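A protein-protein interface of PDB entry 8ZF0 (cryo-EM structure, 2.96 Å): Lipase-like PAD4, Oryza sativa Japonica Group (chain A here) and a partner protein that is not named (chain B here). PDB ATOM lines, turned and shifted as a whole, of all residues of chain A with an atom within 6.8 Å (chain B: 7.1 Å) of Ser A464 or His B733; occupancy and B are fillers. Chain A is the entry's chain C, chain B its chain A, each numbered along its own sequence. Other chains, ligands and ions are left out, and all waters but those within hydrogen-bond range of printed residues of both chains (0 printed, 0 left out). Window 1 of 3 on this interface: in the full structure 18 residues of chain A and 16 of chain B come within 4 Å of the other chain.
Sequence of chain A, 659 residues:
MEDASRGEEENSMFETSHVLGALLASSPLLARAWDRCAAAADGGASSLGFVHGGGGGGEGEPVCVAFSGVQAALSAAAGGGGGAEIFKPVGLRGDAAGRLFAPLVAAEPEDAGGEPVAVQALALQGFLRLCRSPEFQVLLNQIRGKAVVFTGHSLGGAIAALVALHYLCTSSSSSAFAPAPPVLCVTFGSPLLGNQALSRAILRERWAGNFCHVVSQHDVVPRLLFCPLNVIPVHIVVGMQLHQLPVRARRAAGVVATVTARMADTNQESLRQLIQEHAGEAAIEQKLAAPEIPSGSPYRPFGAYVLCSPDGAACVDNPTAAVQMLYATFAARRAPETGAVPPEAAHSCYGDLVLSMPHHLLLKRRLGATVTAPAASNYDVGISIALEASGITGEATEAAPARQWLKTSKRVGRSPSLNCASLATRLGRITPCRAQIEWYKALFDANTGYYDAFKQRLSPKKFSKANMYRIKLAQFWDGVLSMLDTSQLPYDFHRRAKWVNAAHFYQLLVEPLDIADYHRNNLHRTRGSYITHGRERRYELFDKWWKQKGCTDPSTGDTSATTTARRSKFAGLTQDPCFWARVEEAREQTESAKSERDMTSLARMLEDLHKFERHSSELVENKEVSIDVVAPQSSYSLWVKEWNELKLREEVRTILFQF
O of Ser B730 sits at hydrogen-bond distance from N of His B707, at 2.8 Å.
The backbone carbonyl oxygen (O) of Pro A460 sits at hydrogen-bond distance from the side-chain hydroxyl (OG) of Ser A464 (3.3 Å).
The side-chain hydroxyl (OG) of Ser A464 sits at hydrogen-bond distance from the backbone carbonyl oxygen (O) of Lys A461 (3.4 Å).
The side-chain hydroxyl of Ser A464 lies within hydrogen-bond range of a ring nitrogen (NE2) of His B707, 3.3 Å away.
A ring nitrogen (ND1) of His B733 sits at hydrogen-bond distance from the side-chain amide nitrogen (ND2) of Asn A467 (3.1 Å).
Hydrophobic or aromatic side chains of chain B within 4 Å of the printed part of chain A: His B707, Ile B709, His B733 and Pro B757.
Along chain A the printed residues that touch a printed residue of chain B span positions 460 to 471.
Among the printed residues, 7 pairs touch across the chains.
Among the printed residues, no Asp or Glu carboxylate lies within 4 Å of a Lys or Arg side-chain nitrogen of the other chain.
Of chain B, only His B707 (3.3 Å) and His B733 (3.4 Å) come within 4 Å of Ser A464.
Of the printed residues of chain B, Asn A467 touches His B733 (3.1 Å).
Printed residues of chain B within 4 Å of Met A468: His B733 and Pro B757.
Of the printed residues of chain B, Ile A471 touches Pro B757.
Printed residues of chain A within 4 Å of His B707: Ser A464 (3.3 Å).
Of the printed residues of chain A, Ile B709 touches Pro A460 (3.7 Å).
His B733 touches just these residues of chain A: Ser A464, Asn A467 and Met A468.
The nearest residue of chain B that does not touch Ser A464 is Asn B731 (4.2 Å).
The nearest residue of chain A that does not touch His B733 is Ile A471 (5.0 Å).
The nearest printed residue of chain B that does not touch Met A468 is Ala B755 (4.9 Å).
Among the printed residues, pairs that only touch across the chains: Pro A460 with Ile B709, Ser A464 with His B733, Met A468 with His B733, Met A468 with Pro B757 and Ile A471 with Pro B757.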
ATOM      1  N   PHE A 454      10.596  22.326   1.176  1.00  0.00           N
ATOM      2  CA  PHE A 454      11.322  22.184  -0.081  1.00  0.00           C
ATOM      3  C   PHE A 454      11.325  23.489  -0.868  1.00  0.00           C
ATOM      4  O   PHE A 454      12.346  23.862  -1.457  1.00  0.00           O
ATOM      5  CB  PHE A 454      10.714  21.056  -0.914  1.00  0.00           C
ATOM      6  CG  PHE A 454      11.670  20.450  -1.901  1.00  0.00           C
ATOM      7  CD1 PHE A 454      12.685  19.610  -1.476  1.00  0.00           C
ATOM      8  CD2 PHE A 454      11.554  20.720  -3.253  1.00  0.00           C
ATOM      9  CE1 PHE A 454      13.566  19.051  -2.382  1.00  0.00           C
ATOM     10  CE2 PHE A 454      12.431  20.164  -4.165  1.00  0.00           C
ATOM     11  CZ  PHE A 454      13.438  19.328  -3.728  1.00  0.00           C
ATOM     12  N   SER A 459      16.859  23.924   5.906  1.00  0.00           N
ATOM     13  CA  SER A 459      17.825  22.865   6.184  1.00  0.00           C
ATOM     14  C   SER A 459      18.473  22.394   4.888  1.00  0.00           C
ATOM     15  O   SER A 459      18.159  21.301   4.397  1.00  0.00           O
ATOM     16  CB  SER A 459      17.158  21.695   6.910  1.00  0.00           C
ATOM     17  OG  SER A 459      18.092  20.663   7.177  1.00  0.00           O
ATOM     18  N   PRO A 460      19.369  23.193   4.299  1.00  0.00           N
ATOM     19  CA  PRO A 460      19.916  22.843   2.977  1.00  0.00           C
ATOM     20  C   PRO A 460      20.629  21.502   2.935  1.00  0.00           C
ATOM     21  O   PRO A 460      20.627  20.847   1.885  1.00  0.00           O
ATOM     22  CB  PRO A 460      20.881  24.001   2.683  1.00  0.00           C
ATOM     23  CG  PRO A 460      20.411  25.124   3.551  1.00  0.00           C
ATOM     24  CD  PRO A 460      19.905  24.470   4.798  1.00  0.00           C
ATOM     25  N   LYS A 461      21.242  21.072   4.042  1.00  0.00           N
ATOM     26  CA  LYS A 461      21.963  19.804   4.047  1.00  0.00           C
ATOM     27  C   LYS A 461      21.042  18.614   3.812  1.00  0.00           C
ATOM     28  O   LYS A 461      21.517  17.550   3.401  1.00  0.00           O
ATOM     29  CB  LYS A 461      22.719  19.637   5.365  1.00  0.00           C
ATOM     30  CG  LYS A 461      23.978  20.485   5.456  1.00  0.00           C
ATOM     31  CD  LYS A 461      24.846  20.078   6.634  1.00  0.00           C
ATOM     32  CE  LYS A 461      26.196  20.776   6.585  1.00  0.00           C
ATOM     33  NZ  LYS A 461      27.064  20.396   7.732  1.00  0.00           N
ATOM     34  N   LYS A 462      19.744  18.767   4.063  1.00  0.00           N
ATOM     35  CA  LYS A 462      18.758  17.747   3.728  1.00  0.00           C
ATOM     36  C   LYS A 462      18.015  18.051   2.437  1.00  0.00           C
ATOM     37  O   LYS A 462      17.601  17.121   1.733  1.00  0.00           O
ATOM     38  CB  LYS A 462      17.747  17.596   4.870  1.00  0.00           C
ATOM     39  CG  LYS A 462      18.386  17.380   6.232  1.00  0.00           C
ATOM     40  CD  LYS A 462      17.359  17.462   7.348  1.00  0.00           C
ATOM     41  CE  LYS A 462      18.031  17.519   8.710  1.00  0.00           C
ATOM     42  NZ  LYS A 462      17.050  17.744   9.806  1.00  0.00           N
ATOM     43  N   PHE A 463      17.844  19.335   2.114  1.00  0.00           N
ATOM     44  CA  PHE A 463      17.208  19.712   0.857  1.00  0.00           C
ATOM     45  C   PHE A 463      18.029  19.239  -0.335  1.00  0.00           C
ATOM     46  O   PHE A 463      17.471  18.821  -1.355  1.00  0.00           O
ATOM     47  CB  PHE A 463      17.003  21.225   0.807  1.00  0.00           C
ATOM     48  CG  PHE A 463      16.908  21.782  -0.584  1.00  0.00           C
ATOM     49  CD1 PHE A 463      15.775  21.575  -1.352  1.00  0.00           C
ATOM     50  CD2 PHE A 463      17.953  22.515  -1.124  1.00  0.00           C
ATOM     51  CE1 PHE A 463      15.686  22.086  -2.633  1.00  0.00           C
ATOM     52  CE2 PHE A 463      17.869  23.028  -2.403  1.00  0.00           C
ATOM     53  CZ  PHE A 463      16.733  22.813  -3.158  1.00  0.00           C
ATOM     54  N   SER A 464      19.360  19.304  -0.228  1.00  0.00           N
ATOM     55  CA  SER A 464      20.211  18.820  -1.312  1.00  0.00           C
ATOM     56  C   SER A 464      20.028  17.323  -1.532  1.00  0.00           C
ATOM     57  O   SER A 464      19.940  16.862  -2.676  1.00  0.00           O
ATOM     58  CB  SER A 464      21.674  19.145  -1.013  1.00  0.00           C
ATOM     59  OG  SER A 464      22.110  18.494   0.167  1.00  0.00           O
ATOM     60  N   LYS A 465      19.968  16.547  -0.446  1.00  0.00           N
ATOM     61  CA  LYS A 465      19.744  15.110  -0.572  1.00  0.00           C
ATOM     62  C   LYS A 465      18.375  14.816  -1.175  1.00  0.00           C
ATOM     63  O   LYS A 465      18.238  13.929  -2.030  1.00  0.00           O
ATOM     64  CB  LYS A 465      19.883  14.441   0.796  1.00  0.00           C
ATOM     65  CG  LYS A 465      20.379  13.008   0.745  1.00  0.00           C
ATOM     66  CD  LYS A 465      21.885  12.950   0.549  1.00  0.00           C
ATOM     67  CE  LYS A 465      22.433  11.580   0.913  1.00  0.00           C
ATOM     68  NZ  LYS A 465      23.919  11.535   0.823  1.00  0.00           N
ATOM     69  N   ALA A 466      17.348  15.551  -0.738  1.00  0.00           N
ATOM     70  CA  ALA A 466      16.015  15.362  -1.299  1.00  0.00           C
ATOM     71  C   ALA A 466      15.995  15.677  -2.790  1.00  0.00           C
ATOM     72  O   ALA A 466      15.381  14.948  -3.579  1.00  0.00           O
ATOM     73  CB  ALA A 466      15.002  16.229  -0.551  1.00  0.00           C
ATOM     74  N   ASN A 467      16.665  16.759  -3.193  1.00  0.00           N
ATOM     75  CA  ASN A 467      16.733  17.110  -4.607  1.00  0.00           C
ATOM     76  C   ASN A 467      17.477  16.047  -5.405  1.00  0.00           C
ATOM     77  O   ASN A 467      17.078  15.711  -6.526  1.00  0.00           O
ATOM     78  CB  ASN A 467      17.402  18.475  -4.774  1.00  0.00           C
ATOM     79  CG  ASN A 467      17.112  19.106  -6.120  1.00  0.00           C
ATOM     80  OD1 ASN A 467      15.957  19.348  -6.470  1.00  0.00           O
ATOM     81  ND2 ASN A 467      18.163  19.378  -6.885  1.00  0.00           N
ATOM     82  N   MET A 468      18.565  15.511  -4.846  1.00  0.00           N
ATOM     83  CA  MET A 468      19.303  14.447  -5.521  1.00  0.00           C
ATOM     84  C   MET A 468      18.420  13.227  -5.748  1.00  0.00           C
ATOM     85  O   MET A 468      18.385  12.662  -6.849  1.00  0.00           O
ATOM     86  CB  MET A 468      20.536  14.070  -4.700  1.00  0.00           C
ATOM     87  CG  MET A 468      21.847  14.608  -5.240  1.00  0.00           C
ATOM     88  SD  MET A 468      22.318  13.832  -6.796  1.00  0.00           S
ATOM     89  CE  MET A 468      22.819  15.264  -7.741  1.00  0.00           C
ATOM     90  N   TYR A 469      17.691  12.809  -4.711  1.00  0.00           N
ATOM     91  CA  TYR A 469      16.822  11.644  -4.847  1.00  0.00           C
ATOM     92  C   TYR A 469      15.691  11.907  -5.837  1.00  0.00           C
ATOM     93  O   TYR A 469      15.328  11.021  -6.621  1.00  0.00           O
ATOM     94  CB  TYR A 469      16.270  11.239  -3.482  1.00  0.00           C
ATOM     95  CG  TYR A 469      17.314  10.634  -2.571  1.00  0.00           C
ATOM     96  CD1 TYR A 469      18.243   9.725  -3.059  1.00  0.00           C
ATOM     97  CD2 TYR A 469      17.373  10.974  -1.226  1.00  0.00           C
ATOM     98  CE1 TYR A 469      19.201   9.170  -2.233  1.00  0.00           C
ATOM     99  CE2 TYR A 469      18.328  10.423  -0.394  1.00  0.00           C
ATOM    100  CZ  TYR A 469      19.239   9.523  -0.902  1.00  0.00           C
ATOM    101  OH  TYR A 469      20.191   8.971  -0.076  1.00  0.00           O
ATOM    102  N   ILE A 471      15.802  13.947  -8.432  1.00  0.00           N
ATOM    103  CA  ILE A 471      16.387  13.925  -9.770  1.00  0.00           C
ATOM    104  C   ILE A 471      16.633  12.492 -10.222  1.00  0.00           C
ATOM    105  O   ILE A 471      16.370  12.137 -11.378  1.00  0.00           O
ATOM    106  CB  ILE A 471      17.678  14.764  -9.806  1.00  0.00           C
ATOM    107  CG1 ILE A 471      17.351  16.249  -9.640  1.00  0.00           C
ATOM    108  CG2 ILE A 471      18.435  14.531 -11.103  1.00  0.00           C
ATOM    109  CD1 ILE A 471      18.573  17.134  -9.540  1.00  0.00           C
ATOM    110  N   HIS B 707      28.519  22.678  -0.333  1.00  0.00           N
ATOM    111  CA  HIS B 707      27.109  22.983  -0.081  1.00  0.00           C
ATOM    112  C   HIS B 707      26.781  24.443  -0.385  1.00  0.00           C
ATOM    113  O   HIS B 707      26.047  25.101   0.355  1.00  0.00           O
ATOM    114  CB  HIS B 707      26.718  22.627   1.355  1.00  0.00           C
ATOM    115  CG  HIS B 707      26.183  21.238   1.506  1.00  0.00           C
ATOM    116  ND1 HIS B 707      26.801  20.283   2.285  1.00  0.00           N
ATOM    117  CD2 HIS B 707      25.089  20.641   0.977  1.00  0.00           C
ATOM    118  CE1 HIS B 707      26.110  19.158   2.230  1.00  0.00           C
ATOM    119  NE2 HIS B 707      25.067  19.349   1.443  1.00  0.00           N
ATOM    120  N   CYS B 708      27.326  24.956  -1.486  1.00  0.00           N
ATOM    121  CA  CYS B 708      27.010  26.313  -1.923  1.00  0.00           C
ATOM    122  C   CYS B 708      25.633  26.315  -2.573  1.00  0.00           C
ATOM    123  O   CYS B 708      25.472  25.851  -3.706  1.00  0.00           O
ATOM    124  CB  CYS B 708      28.077  26.821  -2.886  1.00  0.00           C
ATOM    125  SG  CYS B 708      28.032  28.606  -3.163  1.00  0.00           S
ATOM    126  N   ILE B 709      24.635  26.831  -1.851  1.00  0.00           N
ATOM    127  CA  ILE B 709      23.256  26.760  -2.324  1.00  0.00           C
ATOM    128  C   ILE B 709      23.058  27.585  -3.589  1.00  0.00           C
ATOM    129  O   ILE B 709      22.450  27.111  -4.557  1.00  0.00           O
ATOM    130  CB  ILE B 709      22.295  27.199  -1.203  1.00  0.00           C
ATOM    131  CG1 ILE B 709      22.062  26.050  -0.221  1.00  0.00           C
ATOM    132  CG2 ILE B 709      20.972  27.677  -1.781  1.00  0.00           C
ATOM    133  CD1 ILE B 709      21.669  24.748  -0.886  1.00  0.00           C
ATOM    134  N   ASP B 710      23.570  28.815  -3.617  1.00  0.00           N
ATOM    135  CA  ASP B 710      23.373  29.719  -4.748  1.00  0.00           C
ATOM    136  C   ASP B 710      24.724  30.033  -5.377  1.00  0.00           C
ATOM    137  O   ASP B 710      25.497  30.830  -4.836  1.00  0.00           O
ATOM    138  CB  ASP B 710      22.660  31.000  -4.308  1.00  0.00           C
ATOM    139  CG  ASP B 710      23.242  31.586  -3.036  1.00  0.00           C
ATOM    140  OD1 ASP B 710      23.246  30.884  -2.004  1.00  0.00           O
ATOM    141  OD2 ASP B 710      23.695  32.749  -3.070  1.00  0.00           O
ATOM    142  N   LEU B 711      25.007  29.403  -6.517  1.00  0.00           N
ATOM    143  CA  LEU B 711      26.228  29.675  -7.264  1.00  0.00           C
ATOM    144  C   LEU B 711      26.031  29.338  -8.736  1.00  0.00           C
ATOM    145  O   LEU B 711      26.103  28.168  -9.125  1.00  0.00           O
ATOM    146  CB  LEU B 711      27.400  28.881  -6.683  1.00  0.00           C
ATOM    147  CG  LEU B 711      28.758  29.058  -7.365  1.00  0.00           C
ATOM    148  CD1 LEU B 711      29.255  30.486  -7.208  1.00  0.00           C
ATOM    149  CD2 LEU B 711      29.768  28.070  -6.805  1.00  0.00           C
ATOM    150  N   SER B 730      31.842  20.790  -3.886  1.00  0.00           N
ATOM    151  CA  SER B 730      31.025  19.705  -3.364  1.00  0.00           C
ATOM    152  C   SER B 730      29.600  20.183  -3.128  1.00  0.00           C
ATOM    153  O   SER B 730      29.391  21.270  -2.578  1.00  0.00           O
ATOM    154  CB  SER B 730      31.613  19.156  -2.059  1.00  0.00           C
ATOM    155  OG  SER B 730      30.663  18.367  -1.364  1.00  0.00           O
ATOM    156  N   ASN B 731      28.633  19.362  -3.540  1.00  0.00           N
ATOM    157  CA  ASN B 731      27.214  19.580  -3.248  1.00  0.00           C
ATOM    158  C   ASN B 731      26.740  20.957  -3.705  1.00  0.00           C
ATOM    159  O   ASN B 731      26.026  21.660  -2.986  1.00  0.00           O
ATOM    160  CB  ASN B 731      26.925  19.375  -1.759  1.00  0.00           C
ATOM    161  CG  ASN B 731      26.586  17.936  -1.426  1.00  0.00           C
ATOM    162  OD1 ASN B 731      25.576  17.402  -1.886  1.00  0.00           O
ATOM    163  ND2 ASN B 731      27.430  17.299  -0.624  1.00  0.00           N
ATOM    164  N   CYS B 732      27.137  21.350  -4.912  1.00  0.00           N
ATOM    165  CA  CYS B 732      26.689  22.595  -5.526  1.00  0.00           C
ATOM    166  C   CYS B 732      25.706  22.239  -6.634  1.00  0.00           C
ATOM    167  O   CYS B 732      26.104  21.718  -7.681  1.00  0.00           O
ATOM    168  CB  CYS B 732      27.870  23.399  -6.065  1.00  0.00           C
ATOM    169  SG  CYS B 732      27.424  25.022  -6.723  1.00  0.00           S
ATOM    170  N   HIS B 733      24.427  22.523  -6.405  1.00  0.00           N
ATOM    171  CA  HIS B 733      23.368  22.147  -7.331  1.00  0.00           C
ATOM    172  C   HIS B 733      23.045  23.234  -8.346  1.00  0.00           C
ATOM    173  O   HIS B 733      22.134  23.049  -9.161  1.00  0.00           O
ATOM    174  CB  HIS B 733      22.097  21.779  -6.555  1.00  0.00           C
ATOM    175  CG  HIS B 733      22.171  20.449  -5.872  1.00  0.00           C
ATOM    176  ND1 HIS B 733      21.166  19.510  -5.963  1.00  0.00           N
ATOM    177  CD2 HIS B 733      23.128  19.900  -5.088  1.00  0.00           C
ATOM    178  CE1 HIS B 733      21.501  18.440  -5.264  1.00  0.00           C
ATOM    179  NE2 HIS B 733      22.687  18.651  -4.723  1.00  0.00           N
ATOM    180  N   ASP B 734      23.762  24.357  -8.323  1.00  0.00           N
ATOM    181  CA  ASP B 734      23.516  25.450  -9.252  1.00  0.00           C
ATOM    182  C   ASP B 734      24.674  25.712 -10.204  1.00  0.00           C
ATOM    183  O   ASP B 734      24.518  26.513 -11.132  1.00  0.00           O
ATOM    184  CB  ASP B 734      23.194  26.740  -8.483  1.00  0.00           C
ATOM    185  CG  ASP B 734      21.782  26.750  -7.931  1.00  0.00           C
ATOM    186  OD1 ASP B 734      21.033  25.785  -8.190  1.00  0.00           O
ATOM    187  OD2 ASP B 734      21.419  27.725  -7.240  1.00  0.00           O
ATOM    188  N   LEU B 735      25.822  25.071 -10.002  1.00  0.00           N
ATOM    189  CA  LEU B 735      26.983  25.271 -10.866  1.00  0.00           C
ATOM    190  C   LEU B 735      26.698  24.641 -12.224  1.00  0.00           C
ATOM    191  O   LEU B 735      26.761  23.420 -12.384  1.00  0.00           O
ATOM    192  CB  LEU B 735      28.230  24.669 -10.228  1.00  0.00           C
ATOM    193  CG  LEU B 735      29.557  24.930 -10.941  1.00  0.00           C
ATOM    194  CD1 LEU B 735      29.830  26.422 -11.040  1.00  0.00           C
ATOM    195  CD2 LEU B 735      30.694  24.220 -10.224  1.00  0.00           C
ATOM    196  N   THR B 736      26.389  25.479 -13.213  1.00  0.00           N
ATOM    197  CA  THR B 736      26.011  24.973 -14.528  1.00  0.00           C
ATOM    198  C   THR B 736      27.232  24.599 -15.360  1.00  0.00           C
ATOM    199  O   THR B 736      27.289  23.508 -15.936  1.00  0.00           O
ATOM    200  CB  THR B 736      25.161  26.008 -15.266  1.00  0.00           C
ATOM    201  OG1 THR B 736      25.804  27.287 -15.209  1.00  0.00           O
ATOM    202  CG2 THR B 736      23.781  26.111 -14.634  1.00  0.00           C
ATOM    203  N   ALA B 755      28.750  15.764  -6.906  1.00  0.00           N
ATOM    204  CA  ALA B 755      27.417  16.186  -6.474  1.00  0.00           C
ATOM    205  C   ALA B 755      27.050  17.544  -7.073  1.00  0.00           C
ATOM    206  O   ALA B 755      26.664  18.480  -6.370  1.00  0.00           O
ATOM    207  CB  ALA B 755      27.309  16.208  -4.947  1.00  0.00           C
ATOM    208  N   CYS B 756      27.176  17.643  -8.396  1.00  0.00           N
ATOM    209  CA  CYS B 756      26.854  18.858  -9.144  1.00  0.00           C
ATOM    210  C   CYS B 756      25.920  18.485 -10.287  1.00  0.00           C
ATOM    211  O   CYS B 756      26.357  18.323 -11.435  1.00  0.00           O
ATOM    212  CB  CYS B 756      28.119  19.545  -9.658  1.00  0.00           C
ATOM    213  SG  CYS B 756      29.189  20.208  -8.362  1.00  0.00           S
ATOM    214  N   PRO B 757      24.624  18.328 -10.005  1.00  0.00           N
ATOM    215  CA  PRO B 757      23.683  17.943 -11.071  1.00  0.00           C
ATOM    216  C   PRO B 757      23.593  18.953 -12.201  1.00  0.00           C
ATOM    217  O   PRO B 757      23.366  18.558 -13.352  1.00  0.00           O
ATOM    218  CB  PRO B 757      22.348  17.812 -10.325  1.00  0.00           C
ATOM    219  CG  PRO B 757      22.502  18.686  -9.123  1.00  0.00           C
ATOM    220  CD  PRO B 757      23.943  18.571  -8.722  1.00  0.00           C
ATOM    221  N   ALA B 758      23.757  20.244 -11.908  1.00  0.00           N
ATOM    222  CA  ALA B 758      23.620  21.263 -12.945  1.00  0.00           C
ATOM    223  C   ALA B 758      24.727  21.169 -13.987  1.00  0.00           C
ATOM    224  O   ALA B 758      24.505  21.512 -15.154  1.00  0.00           O
ATOM    225  CB  ALA B 758      23.602  22.655 -12.313  1.00  0.00           C
ATOM    226  N   LEU B 759      25.916  20.720 -13.591  1.00  0.00           N
ATOM    227  CA  LEU B 759      27.021  20.588 -14.532  1.00  0.00           C
ATOM    228  C   LEU B 759      26.696  19.533 -15.582  1.00  0.00           C
ATOM    229  O   LEU B 759      26.213  18.444 -15.257  1.00  0.00           O
ATOM    230  CB  LEU B 759      28.305  20.222 -13.792  1.00  0.00           C
ATOM    231  CG  LEU B 759      29.579  20.150 -14.637  1.00  0.00           C
ATOM    232  CD1 LEU B 759      30.107  21.546 -14.928  1.00  0.00           C
ATOM    233  CD2 LEU B 759      30.635  19.305 -13.945  1.00  0.00           C
